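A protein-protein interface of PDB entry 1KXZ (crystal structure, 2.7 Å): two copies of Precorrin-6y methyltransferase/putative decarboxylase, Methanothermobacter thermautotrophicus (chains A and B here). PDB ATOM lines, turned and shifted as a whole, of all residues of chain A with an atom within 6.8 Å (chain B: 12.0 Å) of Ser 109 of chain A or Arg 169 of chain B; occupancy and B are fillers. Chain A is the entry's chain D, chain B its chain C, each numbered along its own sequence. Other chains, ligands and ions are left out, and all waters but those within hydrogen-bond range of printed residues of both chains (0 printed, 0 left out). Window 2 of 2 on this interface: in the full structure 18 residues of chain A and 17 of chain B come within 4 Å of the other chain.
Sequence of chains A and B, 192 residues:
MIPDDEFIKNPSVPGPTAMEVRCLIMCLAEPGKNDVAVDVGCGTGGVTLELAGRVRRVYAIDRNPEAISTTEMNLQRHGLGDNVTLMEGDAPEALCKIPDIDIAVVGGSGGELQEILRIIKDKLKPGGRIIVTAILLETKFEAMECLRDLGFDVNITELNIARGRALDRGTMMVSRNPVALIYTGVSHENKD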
ATOM      1  N   PRO A  14     -19.320  24.671 -35.067  1.00  0.00           N
ATOM      2  CA  PRO A  14     -18.688  23.442 -34.595  1.00  0.00           C
ATOM      3  C   PRO A  14     -19.733  22.377 -34.202  1.00  0.00           C
ATOM      4  O   PRO A  14     -20.848  22.697 -33.743  1.00  0.00           O
ATOM      5  CB  PRO A  14     -17.887  23.935 -33.389  1.00  0.00           C
ATOM      6  CG  PRO A  14     -18.707  25.118 -32.902  1.00  0.00           C
ATOM      7  CD  PRO A  14     -18.990  25.805 -34.185  1.00  0.00           C
ATOM      8  N   VAL A  40     -26.367  25.234 -23.330  1.00  0.00           N
ATOM      9  CA  VAL A  40     -25.636  26.457 -23.599  1.00  0.00           C
ATOM     10  C   VAL A  40     -24.590  26.188 -24.645  1.00  0.00           C
ATOM     11  O   VAL A  40     -23.766  25.324 -24.473  1.00  0.00           O
ATOM     12  CB  VAL A  40     -24.966  26.977 -22.351  1.00  0.00           C
ATOM     13  CG1 VAL A  40     -24.292  28.267 -22.648  1.00  0.00           C
ATOM     14  CG2 VAL A  40     -25.982  27.133 -21.229  1.00  0.00           C
ATOM     15  N   GLY A  41     -24.627  26.937 -25.731  1.00  0.00           N
ATOM     16  CA  GLY A  41     -23.679  26.729 -26.802  1.00  0.00           C
ATOM     17  C   GLY A  41     -24.125  25.475 -27.520  1.00  0.00           C
ATOM     18  O   GLY A  41     -23.382  24.502 -27.602  1.00  0.00           O
ATOM     19  N   VAL A 106     -23.549  22.613 -20.624  1.00  0.00           N
ATOM     20  CA  VAL A 106     -22.835  23.767 -21.084  1.00  0.00           C
ATOM     21  C   VAL A 106     -21.679  23.348 -21.973  1.00  0.00           C
ATOM     22  O   VAL A 106     -20.725  22.782 -21.493  1.00  0.00           O
ATOM     23  CB  VAL A 106     -22.235  24.489 -19.915  1.00  0.00           C
ATOM     24  CG1 VAL A 106     -21.664  25.806 -20.365  1.00  0.00           C
ATOM     25  CG2 VAL A 106     -23.257  24.650 -18.807  1.00  0.00           C
ATOM     26  N   GLY A 107     -21.780  23.575 -23.271  1.00  0.00           N
ATOM     27  CA  GLY A 107     -20.681  23.237 -24.161  1.00  0.00           C
ATOM     28  C   GLY A 107     -19.843  24.488 -24.427  1.00  0.00           C
ATOM     29  O   GLY A 107     -18.671  24.599 -24.006  1.00  0.00           O
ATOM     30  N   GLY A 108     -20.494  25.465 -25.065  1.00  0.00           N
ATOM     31  CA  GLY A 108     -19.873  26.736 -25.402  1.00  0.00           C
ATOM     32  C   GLY A 108     -19.158  27.465 -24.275  1.00  0.00           C
ATOM     33  O   GLY A 108     -19.774  28.196 -23.485  1.00  0.00           O
ATOM     34  N   SER A 109     -17.848  27.234 -24.207  1.00  0.00           N
ATOM     35  CA  SER A 109     -16.968  27.866 -23.228  1.00  0.00           C
ATOM     36  C   SER A 109     -17.264  29.372 -23.277  1.00  0.00           C
ATOM     37  O   SER A 109     -17.514  30.001 -22.248  1.00  0.00           O
ATOM     38  CB  SER A 109     -15.497  27.595 -23.604  1.00  0.00           C
ATOM     39  OG  SER A 109     -15.229  27.893 -24.983  1.00  0.00           O
ATOM     40  N   GLY A 110     -17.272  29.906 -24.505  1.00  0.00           N
ATOM     41  CA  GLY A 110     -17.539  31.310 -24.767  1.00  0.00           C
ATOM     42  C   GLY A 110     -16.900  32.272 -23.788  1.00  0.00           C
ATOM     43  O   GLY A 110     -17.449  33.351 -23.577  1.00  0.00           O
ATOM     44  N   GLY A 111     -15.724  31.929 -23.249  1.00  0.00           N
ATOM     45  CA  GLY A 111     -15.053  32.781 -22.269  1.00  0.00           C
ATOM     46  C   GLY A 111     -15.759  32.831 -20.918  1.00  0.00           C
ATOM     47  O   GLY A 111     -15.267  32.287 -19.912  1.00  0.00           O
ATOM     48  N   GLU A 112     -16.940  33.449 -20.928  1.00  0.00           N
ATOM     49  CA  GLU A 112     -17.837  33.641 -19.786  1.00  0.00           C
ATOM     50  C   GLU A 112     -18.385  32.372 -19.105  1.00  0.00           C
ATOM     51  O   GLU A 112     -19.466  32.400 -18.521  1.00  0.00           O
ATOM     52  CB  GLU A 112     -19.010  34.493 -20.261  1.00  0.00           C
ATOM     53  CG  GLU A 112     -19.794  33.818 -21.397  1.00  0.00           C
ATOM     54  CD  GLU A 112     -20.545  34.793 -22.302  1.00  0.00           C
ATOM     55  OE1 GLU A 112     -21.118  34.340 -23.328  1.00  0.00           O
ATOM     56  OE2 GLU A 112     -20.555  36.003 -21.984  1.00  0.00           O
ATOM     57  N   LEU A 113     -17.614  31.291 -19.105  1.00  0.00           N
ATOM     58  CA  LEU A 113     -18.031  30.039 -18.496  1.00  0.00           C
ATOM     59  C   LEU A 113     -18.367  30.201 -17.033  1.00  0.00           C
ATOM     60  O   LEU A 113     -19.423  29.784 -16.564  1.00  0.00           O
ATOM     61  CB  LEU A 113     -16.919  29.021 -18.614  1.00  0.00           C
ATOM     62  CG  LEU A 113     -17.169  27.714 -17.887  1.00  0.00           C
ATOM     63  CD1 LEU A 113     -18.378  26.988 -18.468  1.00  0.00           C
ATOM     64  CD2 LEU A 113     -15.942  26.891 -18.009  1.00  0.00           C
ATOM     65  N   GLN A 114     -17.448  30.796 -16.302  1.00  0.00           N
ATOM     66  CA  GLN A 114     -17.649  31.005 -14.895  1.00  0.00           C
ATOM     67  C   GLN A 114     -18.939  31.770 -14.593  1.00  0.00           C
ATOM     68  O   GLN A 114     -19.632  31.467 -13.622  1.00  0.00           O
ATOM     69  CB  GLN A 114     -16.454  31.741 -14.360  1.00  0.00           C
ATOM     70  CG  GLN A 114     -16.607  32.151 -12.948  1.00  0.00           C
ATOM     71  CD  GLN A 114     -15.963  33.479 -12.720  1.00  0.00           C
ATOM     72  OE1 GLN A 114     -16.588  34.518 -12.924  1.00  0.00           O
ATOM     73  NE2 GLN A 114     -14.672  33.467 -12.394  1.00  0.00           N
ATOM     74  N   ILE A 116     -21.639  31.889 -16.575  1.00  0.00           N
ATOM     75  CA  ILE A 116     -22.721  30.990 -16.932  1.00  0.00           C
ATOM     76  C   ILE A 116     -22.950  29.997 -15.809  1.00  0.00           C
ATOM     77  O   ILE A 116     -24.074  29.757 -15.377  1.00  0.00           O
ATOM     78  CB  ILE A 116     -22.371  30.235 -18.201  1.00  0.00           C
ATOM     79  CG1 ILE A 116     -22.411  31.203 -19.385  1.00  0.00           C
ATOM     80  CG2 ILE A 116     -23.310  29.087 -18.426  1.00  0.00           C
ATOM     81  CD1 ILE A 116     -21.959  30.608 -20.694  1.00  0.00           C
ATOM     82  N   VAL A 132     -20.539  20.057 -18.176  1.00  0.00           N
ATOM     83  CA  VAL A 132     -19.810  20.980 -18.993  1.00  0.00           C
ATOM     84  C   VAL A 132     -18.947  20.135 -19.894  1.00  0.00           C
ATOM     85  O   VAL A 132     -18.196  19.315 -19.411  1.00  0.00           O
ATOM     86  CB  VAL A 132     -18.862  21.816 -18.132  1.00  0.00           C
ATOM     87  CG1 VAL A 132     -18.182  22.855 -18.958  1.00  0.00           C
ATOM     88  CG2 VAL A 132     -19.600  22.432 -16.968  1.00  0.00           C
ATOM     89  N   THR A 133     -19.041  20.363 -21.198  1.00  0.00           N
ATOM     90  CA  THR A 133     -18.285  19.665 -22.235  1.00  0.00           C
ATOM     91  C   THR A 133     -17.107  20.556 -22.490  1.00  0.00           C
ATOM     92  O   THR A 133     -17.256  21.653 -23.008  1.00  0.00           O
ATOM     93  CB  THR A 133     -19.095  19.632 -23.528  1.00  0.00           C
ATOM     94  OG1 THR A 133     -20.388  19.075 -23.268  1.00  0.00           O
ATOM     95  CG2 THR A 133     -18.397  18.801 -24.584  1.00  0.00           C
ATOM     96  N   ILE A 135     -13.564  21.265 -24.401  1.00  0.00           N
ATOM     97  CA  ILE A 135     -12.690  21.006 -25.536  1.00  0.00           C
ATOM     98  C   ILE A 135     -11.289  21.566 -25.194  1.00  0.00           C
ATOM     99  O   ILE A 135     -10.261  20.949 -25.483  1.00  0.00           O
ATOM    100  CB  ILE A 135     -13.277  21.703 -26.795  1.00  0.00           C
ATOM    101  CG1 ILE A 135     -14.467  20.902 -27.298  1.00  0.00           C
ATOM    102  CG2 ILE A 135     -12.236  21.900 -27.883  1.00  0.00           C
ATOM    103  CD1 ILE A 135     -14.183  19.396 -27.358  1.00  0.00           C
ATOM    104  N   LEU A 136     -11.277  22.718 -24.535  1.00  0.00           N
ATOM    105  CA  LEU A 136     -10.055  23.398 -24.148  1.00  0.00           C
ATOM    106  C   LEU A 136      -9.553  22.972 -22.808  1.00  0.00           C
ATOM    107  O   LEU A 136     -10.291  22.795 -21.886  1.00  0.00           O
ATOM    108  CB  LEU A 136     -10.257  24.910 -24.123  1.00  0.00           C
ATOM    109  CG  LEU A 136     -10.852  25.467 -25.422  1.00  0.00           C
ATOM    110  CD1 LEU A 136     -11.011  26.956 -25.302  1.00  0.00           C
ATOM    111  CD2 LEU A 136      -9.999  25.137 -26.612  1.00  0.00           C
ATOM    112  N   GLU A 138      -8.132  24.666 -20.676  1.00  0.00           N
ATOM    113  CA  GLU A 138      -8.475  25.687 -19.677  1.00  0.00           C
ATOM    114  C   GLU A 138      -9.883  25.506 -19.124  1.00  0.00           C
ATOM    115  O   GLU A 138     -10.120  25.716 -17.937  1.00  0.00           O
ATOM    116  CB  GLU A 138      -8.377  27.091 -20.268  1.00  0.00           C
ATOM    117  CG  GLU A 138      -6.968  27.521 -20.642  1.00  0.00           C
ATOM    118  CD  GLU A 138      -6.430  26.812 -21.870  1.00  0.00           C
ATOM    119  OE1 GLU A 138      -7.249  26.331 -22.697  1.00  0.00           O
ATOM    120  OE2 GLU A 138      -5.182  26.763 -22.004  1.00  0.00           O
ATOM    121  N   THR A 139     -10.827  25.192 -20.006  1.00  0.00           N
ATOM    122  CA  THR A 139     -12.205  24.951 -19.616  1.00  0.00           C
ATOM    123  C   THR A 139     -12.253  23.742 -18.668  1.00  0.00           C
ATOM    124  O   THR A 139     -13.005  23.770 -17.699  1.00  0.00           O
ATOM    125  CB  THR A 139     -13.065  24.681 -20.847  1.00  0.00           C
ATOM    126  OG1 THR A 139     -12.872  25.729 -21.802  1.00  0.00           O
ATOM    127  CG2 THR A 139     -14.523  24.614 -20.486  1.00  0.00           C
ATOM    128  N   GLY B 164      -1.504  20.185 -27.117  1.00  0.00           N
ATOM    129  CA  GLY B 164      -2.377  21.327 -27.004  1.00  0.00           C
ATOM    130  C   GLY B 164      -2.123  22.262 -28.149  1.00  0.00           C
ATOM    131  O   GLY B 164      -1.011  22.371 -28.612  1.00  0.00           O
ATOM    132  N   ARG B 165      -3.163  22.911 -28.635  1.00  0.00           N
ATOM    133  CA  ARG B 165      -3.036  23.866 -29.714  1.00  0.00           C
ATOM    134  C   ARG B 165      -3.541  25.135 -29.065  1.00  0.00           C
ATOM    135  O   ARG B 165      -4.641  25.165 -28.511  1.00  0.00           O
ATOM    136  CB  ARG B 165      -3.942  23.484 -30.874  1.00  0.00           C
ATOM    137  CG  ARG B 165      -3.942  24.506 -31.988  1.00  0.00           C
ATOM    138  CD  ARG B 165      -5.009  24.261 -33.086  1.00  0.00           C
ATOM    139  NE  ARG B 165      -4.758  23.030 -33.828  1.00  0.00           N
ATOM    140  CZ  ARG B 165      -5.701  22.212 -34.285  1.00  0.00           C
ATOM    141  NH1 ARG B 165      -6.994  22.483 -34.083  1.00  0.00           N
ATOM    142  NH2 ARG B 165      -5.345  21.104 -34.939  1.00  0.00           N
ATOM    143  N   ALA B 166      -2.703  26.156 -29.029  1.00  0.00           N
ATOM    144  CA  ALA B 166      -3.098  27.432 -28.436  1.00  0.00           C
ATOM    145  C   ALA B 166      -4.042  28.181 -29.382  1.00  0.00           C
ATOM    146  O   ALA B 166      -3.770  28.335 -30.578  1.00  0.00           O
ATOM    147  CB  ALA B 166      -1.866  28.287 -28.099  1.00  0.00           C
ATOM    148  N   LEU B 167      -5.203  28.534 -28.852  1.00  0.00           N
ATOM    149  CA  LEU B 167      -6.183  29.288 -29.590  1.00  0.00           C
ATOM    150  C   LEU B 167      -6.277  30.592 -28.791  1.00  0.00           C
ATOM    151  O   LEU B 167      -5.613  30.740 -27.751  1.00  0.00           O
ATOM    152  CB  LEU B 167      -7.511  28.561 -29.556  1.00  0.00           C
ATOM    153  CG  LEU B 167      -7.546  27.125 -30.064  1.00  0.00           C
ATOM    154  CD1 LEU B 167      -8.971  26.641 -29.938  1.00  0.00           C
ATOM    155  CD2 LEU B 167      -7.074  27.000 -31.504  1.00  0.00           C
ATOM    156  N   ASP B 168      -7.062  31.555 -29.270  1.00  0.00           N
ATOM    157  CA  ASP B 168      -7.210  32.807 -28.532  1.00  0.00           C
ATOM    158  C   ASP B 168      -7.936  32.463 -27.256  1.00  0.00           C
ATOM    159  O   ASP B 168      -7.510  32.831 -26.170  1.00  0.00           O
ATOM    160  CB  ASP B 168      -8.021  33.810 -29.338  1.00  0.00           C
ATOM    161  CG  ASP B 168      -7.327  34.213 -30.619  1.00  0.00           C
ATOM    162  OD1 ASP B 168      -8.034  34.491 -31.613  1.00  0.00           O
ATOM    163  OD2 ASP B 168      -6.076  34.245 -30.642  1.00  0.00           O
ATOM    164  N   ARG B 169      -8.987  31.669 -27.425  1.00  0.00           N
ATOM    165  CA  ARG B 169      -9.838  31.204 -26.335  1.00  0.00           C
ATOM    166  C   ARG B 169      -9.091  30.364 -25.281  1.00  0.00           C
ATOM    167  O   ARG B 169      -9.535  30.258 -24.127  1.00  0.00           O
ATOM    168  CB  ARG B 169     -11.022  30.408 -26.929  1.00  0.00           C
ATOM    169  CG  ARG B 169     -10.622  29.401 -28.038  1.00  0.00           C
ATOM    170  CD  ARG B 169     -11.808  28.596 -28.595  1.00  0.00           C
ATOM    171  NE  ARG B 169     -12.624  29.387 -29.518  1.00  0.00           N
ATOM    172  CZ  ARG B 169     -13.952  29.300 -29.644  1.00  0.00           C
ATOM    173  NH1 ARG B 169     -14.657  28.445 -28.899  1.00  0.00           N
ATOM    174  NH2 ARG B 169     -14.588  30.086 -30.511  1.00  0.00           N
ATOM    175  N   GLY B 170      -7.969  29.768 -25.680  1.00  0.00           N
ATOM    176  CA  GLY B 170      -7.191  28.947 -24.770  1.00  0.00           C
ATOM    177  C   GLY B 170      -6.581  27.727 -25.454  1.00  0.00           C
ATOM    178  O   GLY B 170      -6.608  27.610 -26.666  1.00  0.00           O
ATOM    179  N   THR B 171      -5.958  26.862 -24.670  1.00  0.00           N
ATOM    180  CA  THR B 171      -5.335  25.632 -25.140  1.00  0.00           C
ATOM    181  C   THR B 171      -6.321  24.488 -25.267  1.00  0.00           C
ATOM    182  O   THR B 171      -6.986  24.095 -24.314  1.00  0.00           O
ATOM    183  CB  THR B 171      -4.193  25.214 -24.201  1.00  0.00           C
ATOM    184  OG1 THR B 171      -3.186  26.233 -24.213  1.00  0.00           O
ATOM    185  CG2 THR B 171      -3.603  23.901 -24.611  1.00  0.00           C
ATOM    186  N   MET B 172      -6.362  23.925 -26.454  1.00  0.00           N
ATOM    187  CA  MET B 172      -7.253  22.843 -26.772  1.00  0.00           C
ATOM    188  C   MET B 172      -6.470  21.572 -27.027  1.00  0.00           C
ATOM    189  O   MET B 172      -5.491  21.600 -27.745  1.00  0.00           O
ATOM    190  CB  MET B 172      -7.980  23.210 -28.032  1.00  0.00           C
ATOM    191  CG  MET B 172      -8.832  22.105 -28.563  1.00  0.00           C
ATOM    192  SD  MET B 172      -9.257  22.500 -30.418  1.00  0.00           S
ATOM    193  CE  MET B 172      -7.630  23.277 -30.950  1.00  0.00           C
ATOM    194  N   MET B 173      -6.914  20.436 -26.499  1.00  0.00           N
ATOM    195  CA  MET B 173      -6.163  19.183 -26.711  1.00  0.00           C
ATOM    196  C   MET B 173      -6.519  18.567 -28.042  1.00  0.00           C
ATOM    197  O   MET B 173      -7.696  18.335 -28.346  1.00  0.00           O
ATOM    198  CB  MET B 173      -6.421  18.174 -25.583  1.00  0.00           C
ATOM    199  CG  MET B 173      -5.944  18.652 -24.205  1.00  0.00           C
ATOM    200  SD  MET B 173      -4.040  19.308 -24.268  1.00  0.00           S
ATOM    201  CE  MET B 173      -3.164  17.614 -24.413  1.00  0.00           C
ATOM    202  N   VAL B 174      -5.508  18.307 -28.855  1.00  0.00           N
ATOM    203  CA  VAL B 174      -5.744  17.739 -30.167  1.00  0.00           C
ATOM    204  C   VAL B 174      -5.111  16.381 -30.288  1.00  0.00           C
ATOM    205  O   VAL B 174      -3.896  16.249 -30.265  1.00  0.00           O
ATOM    206  CB  VAL B 174      -5.194  18.604 -31.293  1.00  0.00           C
ATOM    207  CG1 VAL B 174      -5.513  17.932 -32.615  1.00  0.00           C
ATOM    208  CG2 VAL B 174      -5.833  19.968 -31.282  1.00  0.00           C
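OE1 of Glu 138 of chain A sits at hydrogen-bond distance from N of Thr 171 of chain B, 2.4 Å away.
O of Met 172 of chain B sits at hydrogen-bond distance from N of Arg 165 of chain B (2.8 Å).
OG of Ser 109 of chain A touches NH1 of Arg 169 of chain B (3.996 Å). CG2 of Ile 135 of chain A touches CG of Met 172 of chain B, at 3.5 Å. N of Met 173 of chain B touches O of Ile 135 of chain A, at 3.5 Å. Leu 167 of chain B touches Leu 136 of chain A (CD1 to CD2, 3.8 Å). Leu 136 of chain A touches Arg 169 of chain B. O of Thr 171 of chain B touches CA of Leu 136 of chain A, 3.2 Å away. CD2 of Leu 136 of chain A touches CB of Met 172 of chain B, at 3.1 Å. Glu 138 of chain A touches Gly 170 of chain B.
Of the printed residues of chain B, Ser 109 of chain A touches Arg 169 (3.996 Å). Printed residues of chain A within 4 Å of Arg 169 of chain B: Ser 109 and Leu 136. Gly 41 of chain A touches none of the printed residues of chain B. No residue of chain B comes within 4 Å of Gly 107 of chain A. No residue of chain B comes within 4 Å of Gly 108 of chain A. No residue of chain B comes within 4 Å of Gly 110 of chain A. No residue of chain B comes within 4 Å of Gly 111 of chain A. Glu 112 of chain A touches none of the printed residues of chain B. Leu 113 of chain A touches none of the printed residues of chain B. Printed residues of chain B within 4 Å of Leu 136 of chain A: Leu 167, Arg 169, Thr 171 and Met 172. Glu 138 of chain A touches just these residues of chain B: Gly 170 and Thr 171. No residue of chain B comes within 4 Å of Thr 139 of chain A. Printed residues of chain A within 4 Å of Thr 171 of chain B: Leu 136 (3.2 Å) and Glu 138 (2.4 Å). Printed residues of chain A within 4 Å of Gly 170 of chain B: Glu 138. Printed residues of chain A within 4 Å of Leu 167 of chain B: Leu 136. Val 132 of chain A touches none of the printed residues of chain B. Gln 114 of chain A touches none of the printed residues of chain B. The nearest printed residue of chain A that does not touch Arg 169 of chain B is Glu 138 of chain A (4.8 Å). The nearest printed residue of chain A that does not touch Gly 170 of chain B is Leu 136 of chain A (4.2 Å).
Of the 11 printed residues of chain B, 6 touch a printed residue of chain A. Hydrophobic or aromatic side chains of chain A within 4 Å of the printed part of chain B: Ile 135 and Leu 136. Along chain A the printed residues that touch a printed residue of chain B span positions 109 to 138.
No position is printed for both chains. Of the 9 pairs that touch across the chains among the printed residues, none has its exchanged pair printed and touching as well.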
